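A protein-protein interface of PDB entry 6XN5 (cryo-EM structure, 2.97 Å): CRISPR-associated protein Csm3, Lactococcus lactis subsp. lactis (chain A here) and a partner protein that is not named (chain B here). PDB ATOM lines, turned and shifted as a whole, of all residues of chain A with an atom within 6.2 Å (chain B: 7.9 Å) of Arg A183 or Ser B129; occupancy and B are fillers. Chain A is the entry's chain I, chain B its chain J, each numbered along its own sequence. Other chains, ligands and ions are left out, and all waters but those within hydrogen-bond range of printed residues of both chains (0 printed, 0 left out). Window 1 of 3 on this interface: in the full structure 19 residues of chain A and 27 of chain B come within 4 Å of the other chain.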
ATOM      1  N   LYS A 118      15.337  13.599  11.810  1.00  0.00           N
ATOM      2  CA  LYS A 118      15.736  12.212  11.958  1.00  0.00           C
ATOM      3  C   LYS A 118      16.434  12.018  13.295  1.00  0.00           C
ATOM      4  O   LYS A 118      17.078  12.931  13.821  1.00  0.00           O
ATOM      5  CB  LYS A 118      16.643  11.757  10.805  1.00  0.00           C
ATOM      6  CG  LYS A 118      17.894  12.585  10.611  1.00  0.00           C
ATOM      7  CD  LYS A 118      18.777  12.000   9.520  1.00  0.00           C
ATOM      8  CE  LYS A 118      19.680  10.912  10.066  1.00  0.00           C
ATOM      9  NZ  LYS A 118      20.754  10.538   9.110  1.00  0.00           N
ATOM     10  N   GLU A 120      19.249  10.673  14.909  1.00  0.00           N
ATOM     11  CA  GLU A 120      20.596  10.204  14.596  1.00  0.00           C
ATOM     12  C   GLU A 120      21.260   9.719  15.881  1.00  0.00           C
ATOM     13  O   GLU A 120      21.801  10.503  16.662  1.00  0.00           O
ATOM     14  CB  GLU A 120      21.405  11.311  13.934  1.00  0.00           C
ATOM     15  CG  GLU A 120      22.607  10.812  13.165  1.00  0.00           C
ATOM     16  CD  GLU A 120      23.853  10.774  14.009  1.00  0.00           C
ATOM     17  OE1 GLU A 120      23.980  11.624  14.913  1.00  0.00           O
ATOM     18  OE2 GLU A 120      24.705   9.895  13.770  1.00  0.00           O
ATOM     19  N   ASN A 121      21.229   8.403  16.092  1.00  0.00           N
ATOM     20  CA  ASN A 121      21.854   7.802  17.262  1.00  0.00           C
ATOM     21  C   ASN A 121      23.376   7.823  17.120  1.00  0.00           C
ATOM     22  O   ASN A 121      23.925   8.066  16.047  1.00  0.00           O
ATOM     23  CB  ASN A 121      21.373   6.364  17.454  1.00  0.00           C
ATOM     24  CG  ASN A 121      19.891   6.201  17.193  1.00  0.00           C
ATOM     25  OD1 ASN A 121      19.481   5.366  16.388  1.00  0.00           O
ATOM     26  ND2 ASN A 121      19.078   6.998  17.872  1.00  0.00           N
ATOM     27  N   GLY A 179      26.192  21.315   5.500  1.00  0.00           N
ATOM     28  CA  GLY A 179      25.657  20.516   6.581  1.00  0.00           C
ATOM     29  C   GLY A 179      26.386  19.205   6.782  1.00  0.00           C
ATOM     30  O   GLY A 179      27.467  18.964   6.248  1.00  0.00           O
ATOM     31  N   HIS A 180      25.739  18.316   7.536  1.00  0.00           N
ATOM     32  CA  HIS A 180      26.308  17.011   7.875  1.00  0.00           C
ATOM     33  C   HIS A 180      26.171  16.038   6.701  1.00  0.00           C
ATOM     34  O   HIS A 180      25.551  14.981   6.793  1.00  0.00           O
ATOM     35  CB  HIS A 180      25.636  16.453   9.123  1.00  0.00           C
ATOM     36  CG  HIS A 180      25.503  17.445  10.233  1.00  0.00           C
ATOM     37  ND1 HIS A 180      24.332  18.126  10.484  1.00  0.00           N
ATOM     38  CD2 HIS A 180      26.396  17.880  11.152  1.00  0.00           C
ATOM     39  CE1 HIS A 180      24.507  18.933  11.514  1.00  0.00           C
ATOM     40  NE2 HIS A 180      25.751  18.805  11.936  1.00  0.00           N
ATOM     41  N   GLY A 181      26.786  16.408   5.587  1.00  0.00           N
ATOM     42  CA  GLY A 181      26.554  15.716   4.342  1.00  0.00           C
ATOM     43  C   GLY A 181      27.451  14.522   4.149  1.00  0.00           C
ATOM     44  O   GLY A 181      27.166  13.645   3.332  1.00  0.00           O
ATOM     45  N   THR A 182      28.536  14.480   4.916  1.00  0.00           N
ATOM     46  CA  THR A 182      29.539  13.441   4.769  1.00  0.00           C
ATOM     47  C   THR A 182      29.013  12.081   5.222  1.00  0.00           C
ATOM     48  O   THR A 182      29.453  11.053   4.700  1.00  0.00           O
ATOM     49  CB  THR A 182      30.790  13.890   5.538  1.00  0.00           C
ATOM     50  OG1 THR A 182      31.238  15.131   4.983  1.00  0.00           O
ATOM     51  CG2 THR A 182      31.942  12.931   5.376  1.00  0.00           C
ATOM     52  N   ARG A 183      28.010  12.057   6.099  1.00  0.00           N
ATOM     53  CA  ARG A 183      27.418  10.801   6.541  1.00  0.00           C
ATOM     54  C   ARG A 183      25.996  10.627   6.014  1.00  0.00           C
ATOM     55  O   ARG A 183      25.116  10.140   6.730  1.00  0.00           O
ATOM     56  CB  ARG A 183      27.430  10.707   8.071  1.00  0.00           C
ATOM     57  CG  ARG A 183      26.862  11.914   8.809  1.00  0.00           C
ATOM     58  CD  ARG A 183      27.427  12.001  10.208  1.00  0.00           C
ATOM     59  NE  ARG A 183      28.822  12.412  10.184  1.00  0.00           N
ATOM     60  CZ  ARG A 183      29.220  13.677  10.219  1.00  0.00           C
ATOM     61  NH1 ARG A 183      28.331  14.655  10.294  1.00  0.00           N
ATOM     62  NH2 ARG A 183      30.507  13.963  10.190  1.00  0.00           N
ATOM     63  N   GLY A 184      25.765  10.991   4.757  1.00  0.00           N
ATOM     64  CA  GLY A 184      24.483  10.715   4.139  1.00  0.00           C
ATOM     65  C   GLY A 184      23.502  11.863   4.080  1.00  0.00           C
ATOM     66  O   GLY A 184      22.340  11.708   4.467  1.00  0.00           O
ATOM     67  N   SER A 185      23.947  13.016   3.591  1.00  0.00           N
ATOM     68  CA  SER A 185      23.055  14.155   3.456  1.00  0.00           C
ATOM     69  C   SER A 185      23.523  15.026   2.302  1.00  0.00           C
ATOM     70  O   SER A 185      24.657  14.912   1.836  1.00  0.00           O
ATOM     71  CB  SER A 185      22.989  14.965   4.752  1.00  0.00           C
ATOM     72  OG  SER A 185      22.237  14.278   5.735  1.00  0.00           O
ATOM     73  N   ARG A 187      22.690  15.730  -1.035  1.00  0.00           N
ATOM     74  CA  ARG A 187      22.984  15.489  -2.444  1.00  0.00           C
ATOM     75  C   ARG A 187      21.937  16.146  -3.334  1.00  0.00           C
ATOM     76  O   ARG A 187      20.733  15.962  -3.137  1.00  0.00           O
ATOM     77  CB  ARG A 187      23.067  13.988  -2.726  1.00  0.00           C
ATOM     78  CG  ARG A 187      24.478  13.412  -2.643  1.00  0.00           C
ATOM     79  CD  ARG A 187      25.012  13.423  -1.224  1.00  0.00           C
ATOM     80  NE  ARG A 187      26.406  13.014  -1.146  1.00  0.00           N
ATOM     81  CZ  ARG A 187      27.157  13.176  -0.064  1.00  0.00           C
ATOM     82  NH1 ARG A 187      26.637  13.737   1.014  1.00  0.00           N
ATOM     83  NH2 ARG A 187      28.422  12.783  -0.066  1.00  0.00           N
ATOM     84  N   ILE B  17      18.414  -0.626  11.982  1.00  0.00           N
ATOM     85  CA  ILE B  17      19.339   0.461  12.283  1.00  0.00           C
ATOM     86  C   ILE B  17      18.615   1.549  13.063  1.00  0.00           C
ATOM     87  O   ILE B  17      18.124   2.522  12.477  1.00  0.00           O
ATOM     88  CB  ILE B  17      19.974   1.043  11.007  1.00  0.00           C
ATOM     89  CG1 ILE B  17      20.498  -0.077  10.116  1.00  0.00           C
ATOM     90  CG2 ILE B  17      21.116   1.983  11.365  1.00  0.00           C
ATOM     91  CD1 ILE B  17      21.586  -0.894  10.746  1.00  0.00           C
ATOM     92  N   TYR B 125      14.558   3.231   4.354  1.00  0.00           N
ATOM     93  CA  TYR B 125      15.872   3.350   3.737  1.00  0.00           C
ATOM     94  C   TYR B 125      16.905   3.215   4.844  1.00  0.00           C
ATOM     95  O   TYR B 125      16.569   3.228   6.030  1.00  0.00           O
ATOM     96  CB  TYR B 125      16.035   4.679   3.000  1.00  0.00           C
ATOM     97  CG  TYR B 125      16.322   5.855   3.904  1.00  0.00           C
ATOM     98  CD1 TYR B 125      15.320   6.414   4.685  1.00  0.00           C
ATOM     99  CD2 TYR B 125      17.592   6.416   3.966  1.00  0.00           C
ATOM    100  CE1 TYR B 125      15.577   7.491   5.510  1.00  0.00           C
ATOM    101  CE2 TYR B 125      17.856   7.491   4.789  1.00  0.00           C
ATOM    102  CZ  TYR B 125      16.846   8.024   5.556  1.00  0.00           C
ATOM    103  OH  TYR B 125      17.110   9.095   6.374  1.00  0.00           O
ATOM    104  N   ILE B 126      18.167   3.098   4.451  1.00  0.00           N
ATOM    105  CA  ILE B 126      19.273   3.012   5.397  1.00  0.00           C
ATOM    106  C   ILE B 126      20.066   4.313   5.311  1.00  0.00           C
ATOM    107  O   ILE B 126      20.574   4.654   4.234  1.00  0.00           O
ATOM    108  CB  ILE B 126      20.165   1.796   5.124  1.00  0.00           C
ATOM    109  CG1 ILE B 126      19.403   0.501   5.414  1.00  0.00           C
ATOM    110  CG2 ILE B 126      21.430   1.869   5.951  1.00  0.00           C
ATOM    111  CD1 ILE B 126      18.906   0.376   6.821  1.00  0.00           C
ATOM    112  N   PRO B 127      20.175   5.081   6.391  1.00  0.00           N
ATOM    113  CA  PRO B 127      20.967   6.315   6.349  1.00  0.00           C
ATOM    114  C   PRO B 127      22.457   6.026   6.274  1.00  0.00           C
ATOM    115  O   PRO B 127      22.941   4.975   6.697  1.00  0.00           O
ATOM    116  CB  PRO B 127      20.605   7.019   7.661  1.00  0.00           C
ATOM    117  CG  PRO B 127      19.347   6.349   8.133  1.00  0.00           C
ATOM    118  CD  PRO B 127      19.439   4.940   7.655  1.00  0.00           C
ATOM    119  N   GLY B 128      23.193   6.997   5.728  1.00  0.00           N
ATOM    120  CA  GLY B 128      24.606   6.802   5.454  1.00  0.00           C
ATOM    121  C   GLY B 128      25.502   6.845   6.669  1.00  0.00           C
ATOM    122  O   GLY B 128      26.658   6.413   6.588  1.00  0.00           O
ATOM    123  N   SER B 129      24.992   7.349   7.795  1.00  0.00           N
ATOM    124  CA  SER B 129      25.776   7.361   9.025  1.00  0.00           C
ATOM    125  C   SER B 129      26.019   5.952   9.547  1.00  0.00           C
ATOM    126  O   SER B 129      27.035   5.704  10.202  1.00  0.00           O
ATOM    127  CB  SER B 129      25.072   8.207  10.080  1.00  0.00           C
ATOM    128  OG  SER B 129      24.704   9.468   9.552  1.00  0.00           O
ATOM    129  N   SER B 130      25.109   5.019   9.254  1.00  0.00           N
ATOM    130  CA  SER B 130      25.311   3.621   9.621  1.00  0.00           C
ATOM    131  C   SER B 130      26.504   3.025   8.887  1.00  0.00           C
ATOM    132  O   SER B 130      27.352   2.352   9.491  1.00  0.00           O
ATOM    133  CB  SER B 130      24.051   2.822   9.308  1.00  0.00           C
ATOM    134  OG  SER B 130      24.035   2.435   7.950  1.00  0.00           O
ATOM    135  N   LEU B 131      26.592   3.274   7.580  1.00  0.00           N
ATOM    136  CA  LEU B 131      27.736   2.804   6.806  1.00  0.00           C
ATOM    137  C   LEU B 131      29.016   3.515   7.214  1.00  0.00           C
ATOM    138  O   LEU B 131      30.094   2.905   7.199  1.00  0.00           O
ATOM    139  CB  LEU B 131      27.476   2.986   5.311  1.00  0.00           C
ATOM    140  CG  LEU B 131      26.847   1.846   4.505  1.00  0.00           C
ATOM    141  CD1 LEU B 131      27.827   0.696   4.437  1.00  0.00           C
ATOM    142  CD2 LEU B 131      25.519   1.369   5.070  1.00  0.00           C
ATOM    143  N   LYS B 132      28.920   4.789   7.601  1.00  0.00           N
ATOM    144  CA  LYS B 132      30.110   5.489   8.069  1.00  0.00           C
ATOM    145  C   LYS B 132      30.590   4.939   9.408  1.00  0.00           C
ATOM    146  O   LYS B 132      31.798   4.840   9.649  1.00  0.00           O
ATOM    147  CB  LYS B 132      29.844   6.987   8.162  1.00  0.00           C
ATOM    148  CG  LYS B 132      31.109   7.779   7.986  1.00  0.00           C
ATOM    149  CD  LYS B 132      30.853   9.238   7.794  1.00  0.00           C
ATOM    150  CE  LYS B 132      32.127   9.909   7.361  1.00  0.00           C
ATOM    151  NZ  LYS B 132      33.327   9.355   8.027  1.00  0.00           N
ATOM    152  N   GLY B 133      29.662   4.553  10.284  1.00  0.00           N
ATOM    153  CA  GLY B 133      30.054   3.888  11.517  1.00  0.00           C
ATOM    154  C   GLY B 133      30.656   2.515  11.278  1.00  0.00           C
ATOM    155  O   GLY B 133      31.592   2.108  11.971  1.00  0.00           O
ATOM    156  N   ALA B 134      30.128   1.787  10.290  1.00  0.00           N
ATOM    157  CA  ALA B 134      30.697   0.490   9.934  1.00  0.00           C
ATOM    158  C   ALA B 134      32.119   0.631   9.395  1.00  0.00           C
ATOM    159  O   ALA B 134      33.008  -0.163   9.735  1.00  0.00           O
ATOM    160  CB  ALA B 134      29.799  -0.204   8.917  1.00  0.00           C
ATOM    161  N   LEU B 135      32.370   1.659   8.587  1.00  0.00           N
ATOM    162  CA  LEU B 135      33.740   1.890   8.138  1.00  0.00           C
ATOM    163  C   LEU B 135      34.608   2.484   9.246  1.00  0.00           C
ATOM    164  O   LEU B 135      35.840   2.408   9.170  1.00  0.00           O
ATOM    165  CB  LEU B 135      33.745   2.774   6.893  1.00  0.00           C
ATOM    166  CG  LEU B 135      32.990   2.134   5.724  1.00  0.00           C
ATOM    167  CD1 LEU B 135      32.605   3.164   4.674  1.00  0.00           C
ATOM    168  CD2 LEU B 135      33.794   0.998   5.107  1.00  0.00           C
ATOM    169  N   ARG B 136      33.993   3.069  10.282  1.00  0.00           N
ATOM    170  CA  ARG B 136      34.755   3.445  11.471  1.00  0.00           C
ATOM    171  C   ARG B 136      35.219   2.215  12.237  1.00  0.00           C
ATOM    172  O   ARG B 136      36.318   2.204  12.802  1.00  0.00           O
ATOM    173  CB  ARG B 136      33.927   4.353  12.382  1.00  0.00           C
ATOM    174  CG  ARG B 136      34.002   5.819  12.017  1.00  0.00           C
ATOM    175  CD  ARG B 136      33.763   6.726  13.212  1.00  0.00           C
ATOM    176  NE  ARG B 136      34.193   8.095  12.938  1.00  0.00           N
ATOM    177  CZ  ARG B 136      35.452   8.519  13.017  1.00  0.00           C
ATOM    178  NH1 ARG B 136      36.422   7.687  13.366  1.00  0.00           N
ATOM    179  NH2 ARG B 136      35.744   9.781  12.747  1.00  0.00           N
ATOM    180  N   PHE B 153      38.637  10.625   8.252  1.00  0.00           N
ATOM    181  CA  PHE B 153      37.239  10.403   7.914  1.00  0.00           C
ATOM    182  C   PHE B 153      36.436  11.683   7.738  1.00  0.00           C
ATOM    183  O   PHE B 153      35.202  11.640   7.813  1.00  0.00           O
ATOM    184  CB  PHE B 153      36.579   9.509   8.961  1.00  0.00           C
ATOM    185  CG  PHE B 153      36.744   8.044   8.689  1.00  0.00           C
ATOM    186  CD1 PHE B 153      37.630   7.597   7.721  1.00  0.00           C
ATOM    187  CD2 PHE B 153      36.018   7.113   9.401  1.00  0.00           C
ATOM    188  CE1 PHE B 153      37.789   6.254   7.473  1.00  0.00           C
ATOM    189  CE2 PHE B 153      36.166   5.766   9.152  1.00  0.00           C
ATOM    190  CZ  PHE B 153      37.051   5.335   8.188  1.00  0.00           C
ATOM    191  N   ALA B 154      37.092  12.816   7.500  1.00  0.00           N
ATOM    192  CA  ALA B 154      36.371  13.959   6.959  1.00  0.00           C
ATOM    193  C   ALA B 154      36.216  13.867   5.450  1.00  0.00           C
ATOM    194  O   ALA B 154      35.395  14.590   4.873  1.00  0.00           O
ATOM    195  CB  ALA B 154      37.076  15.263   7.330  1.00  0.00           C
ATOM    196  N   LEU B 156      35.661  10.848   3.701  1.00  0.00           N
ATOM    197  CA  LEU B 156      34.976   9.625   3.290  1.00  0.00           C
ATOM    198  C   LEU B 156      33.495   9.966   3.126  1.00  0.00           C
ATOM    199  O   LEU B 156      32.706   9.898   4.069  1.00  0.00           O
ATOM    200  CB  LEU B 156      35.257   8.495   4.291  1.00  0.00           C
ATOM    201  CG  LEU B 156      34.776   7.068   4.018  1.00  0.00           C
ATOM    202  CD1 LEU B 156      35.815   6.077   4.473  1.00  0.00           C
ATOM    203  CD2 LEU B 156      33.520   6.808   4.804  1.00  0.00           C
ATOM    204  N   GLN B 157      33.131  10.332   1.900  1.00  0.00           N
ATOM    205  CA  GLN B 157      31.861  10.982   1.579  1.00  0.00           C
ATOM    206  C   GLN B 157      30.811   9.910   1.314  1.00  0.00           C
ATOM    207  O   GLN B 157      30.589   9.519   0.165  1.00  0.00           O
ATOM    208  CB  GLN B 157      32.031  11.855   0.343  1.00  0.00           C
ATOM    209  CG  GLN B 157      32.963  13.037   0.459  1.00  0.00           C
ATOM    210  CD  GLN B 157      32.502  14.028   1.473  1.00  0.00           C
ATOM    211  OE1 GLN B 157      33.095  14.186   2.539  1.00  0.00           O
ATOM    212  NE2 GLN B 157      31.397  14.670   1.173  1.00  0.00           N
ATOM    213  N   VAL B 158      30.143   9.439   2.357  1.00  0.00           N
ATOM    214  CA  VAL B 158      29.107   8.424   2.211  1.00  0.00           C
ATOM    215  C   VAL B 158      27.757   9.119   2.121  1.00  0.00           C
ATOM    216  O   VAL B 158      27.421   9.946   2.974  1.00  0.00           O
ATOM    217  CB  VAL B 158      29.150   7.414   3.371  1.00  0.00           C
ATOM    218  CG1 VAL B 158      27.848   6.646   3.483  1.00  0.00           C
ATOM    219  CG2 VAL B 158      30.277   6.447   3.158  1.00  0.00           C
ATOM    220  N   SER B 159      26.995   8.803   1.076  1.00  0.00           N
ATOM    221  CA  SER B 159      25.663   9.352   0.882  1.00  0.00           C
ATOM    222  C   SER B 159      24.621   8.390   1.447  1.00  0.00           C
ATOM    223  O   SER B 159      24.947   7.389   2.088  1.00  0.00           O
ATOM    224  CB  SER B 159      25.403   9.615  -0.598  1.00  0.00           C
ATOM    225  OG  SER B 159      26.432  10.395  -1.170  1.00  0.00           O
ATOM    226  N   ASP B 160      23.352   8.680   1.202  1.00  0.00           N
ATOM    227  CA  ASP B 160      22.290   7.755   1.551  1.00  0.00           C
ATOM    228  C   ASP B 160      22.113   6.712   0.456  1.00  0.00           C
ATOM    229  O   ASP B 160      22.925   6.580  -0.462  1.00  0.00           O
ATOM    230  CB  ASP B 160      20.972   8.490   1.786  1.00  0.00           C
ATOM    231  CG  ASP B 160      20.897   9.124   3.156  1.00  0.00           C
ATOM    232  OD1 ASP B 160      21.781   8.844   3.987  1.00  0.00           O
ATOM    233  OD2 ASP B 160      19.943   9.887   3.411  1.00  0.00           O
ATOM    234  N   PHE B 199      24.309   2.041  -2.501  1.00  0.00           N
ATOM    235  CA  PHE B 199      24.787   3.257  -1.858  1.00  0.00           C
ATOM    236  C   PHE B 199      25.755   4.000  -2.766  1.00  0.00           C
ATOM    237  O   PHE B 199      26.620   3.387  -3.397  1.00  0.00           O
ATOM    238  CB  PHE B 199      25.502   2.926  -0.552  1.00  0.00           C
ATOM    239  CG  PHE B 199      24.636   3.013   0.665  1.00  0.00           C
ATOM    240  CD1 PHE B 199      24.437   4.223   1.306  1.00  0.00           C
ATOM    241  CD2 PHE B 199      24.061   1.870   1.194  1.00  0.00           C
ATOM    242  CE1 PHE B 199      23.656   4.295   2.436  1.00  0.00           C
ATOM    243  CE2 PHE B 199      23.276   1.936   2.317  1.00  0.00           C
ATOM    244  CZ  PHE B 199      23.080   3.149   2.944  1.00  0.00           C
ATOM    245  N   ILE B 270      27.054  -3.754  10.543  1.00  0.00           N
ATOM    246  CA  ILE B 270      26.315  -2.534  10.837  1.00  0.00           C
ATOM    247  C   ILE B 270      25.443  -2.739  12.067  1.00  0.00           C
ATOM    248  O   ILE B 270      24.984  -3.853  12.352  1.00  0.00           O
ATOM    249  CB  ILE B 270      25.503  -2.090   9.609  1.00  0.00           C
ATOM    250  CG1 ILE B 270      24.492  -3.154   9.189  1.00  0.00           C
ATOM    251  CG2 ILE B 270      26.418  -1.741   8.471  1.00  0.00           C
ATOM    252  CD1 ILE B 270      23.535  -2.682   8.124  1.00  0.00           C
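The side-chain hydroxyl (OG1) of Thr A182 sits at hydrogen-bond distance from the side-chain amide oxygen (OE1) of Gln B157 (3.2 Å). N of Val B158 sits at hydrogen-bond distance from O of Thr A182, at 2.9 Å. O of Arg A183 lies within hydrogen-bond range of OG of Ser B129, 2.9 Å away. The backbone NH (N) of Gly A184 is in hydrogen-bond range of the backbone carbonyl oxygen (O) of Val B158, 2.6 Å away. The side-chain hydroxyl (OG) of Ser B159 sits at hydrogen-bond distance from the guanidinium group (NE) of Arg A187. O of Gly A184 sits close to OD1 of Asp B160, 3.0 Å away.
O of Ser A185 lies within hydrogen-bond range of NH1 of Arg A187. The side-chain hydroxyl (OG) of Ser B130 lies within hydrogen-bond range of the backbone carbonyl oxygen (O) of Pro B127 (3.0 Å). OD1 of Asp B160 is in hydrogen-bond range of N of Gly B128. The backbone carbonyl oxygen (O) of Phe B153 is in hydrogen-bond range of the side-chain amino group (NZ) of Lys B132 (3.0 Å). The backbone carbonyl oxygen (O) of Ala B154 lies close to the side-chain amide oxygen (OE1) of Gln B157 (3.3 Å).
Among the printed residues, merely in contact across the chains: Arg A183 with Gly B128, Thr A182 with Leu B156, Arg A183 with Val B158, Gly A184 with Ser B159, Thr A182 with Lys B132, Gly A181 with Val B158, Arg A187 with Gln B157, Arg A183 with Lys B132, Lys A118 with Pro B127 and Thr A182 with Ala B154.
Printed residues of chain B within 4 Å of Gly A181: Val B158 (3.7 Å). Arg A183 touches just these residues of chain B: Gly B128, Ser B129, Lys B132 and Val B158. Of the printed residues of chain A, Pro B127 touches Lys A118 (3.8 Å). Ser B129 touches just one residue of chain A: Arg A183 (2.9 Å). Printed residues of chain A within 4 Å of Asp B160: Gly A184. The nearest residue of chain A that does not touch Ser B129 is Glu A120 (4.1 Å). The nearest printed residue of chain B that does not touch Gly A184 is Gly B128 (4.1 Å).
Printed residues of chain B that touch a printed residue of chain A: Pro B127, Gly B128, Ser B129, Lys B132, Ala B154, Leu B156, Gln B157, Val B158, Ser B159 and Asp B160. Hydrophobic or aromatic side chains of chain B that line the printed part of chain A: Pro B127 and Val B158. Printed residues of chain A that touch a printed residue of chain B: Lys A118, Gly A181, Thr A182, Arg A183, Gly A184 and Arg A187. Among the printed residues, no Asp or Glu carboxylate lies within 4 Å of a Lys or Arg side-chain nitrogen of the other chain.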
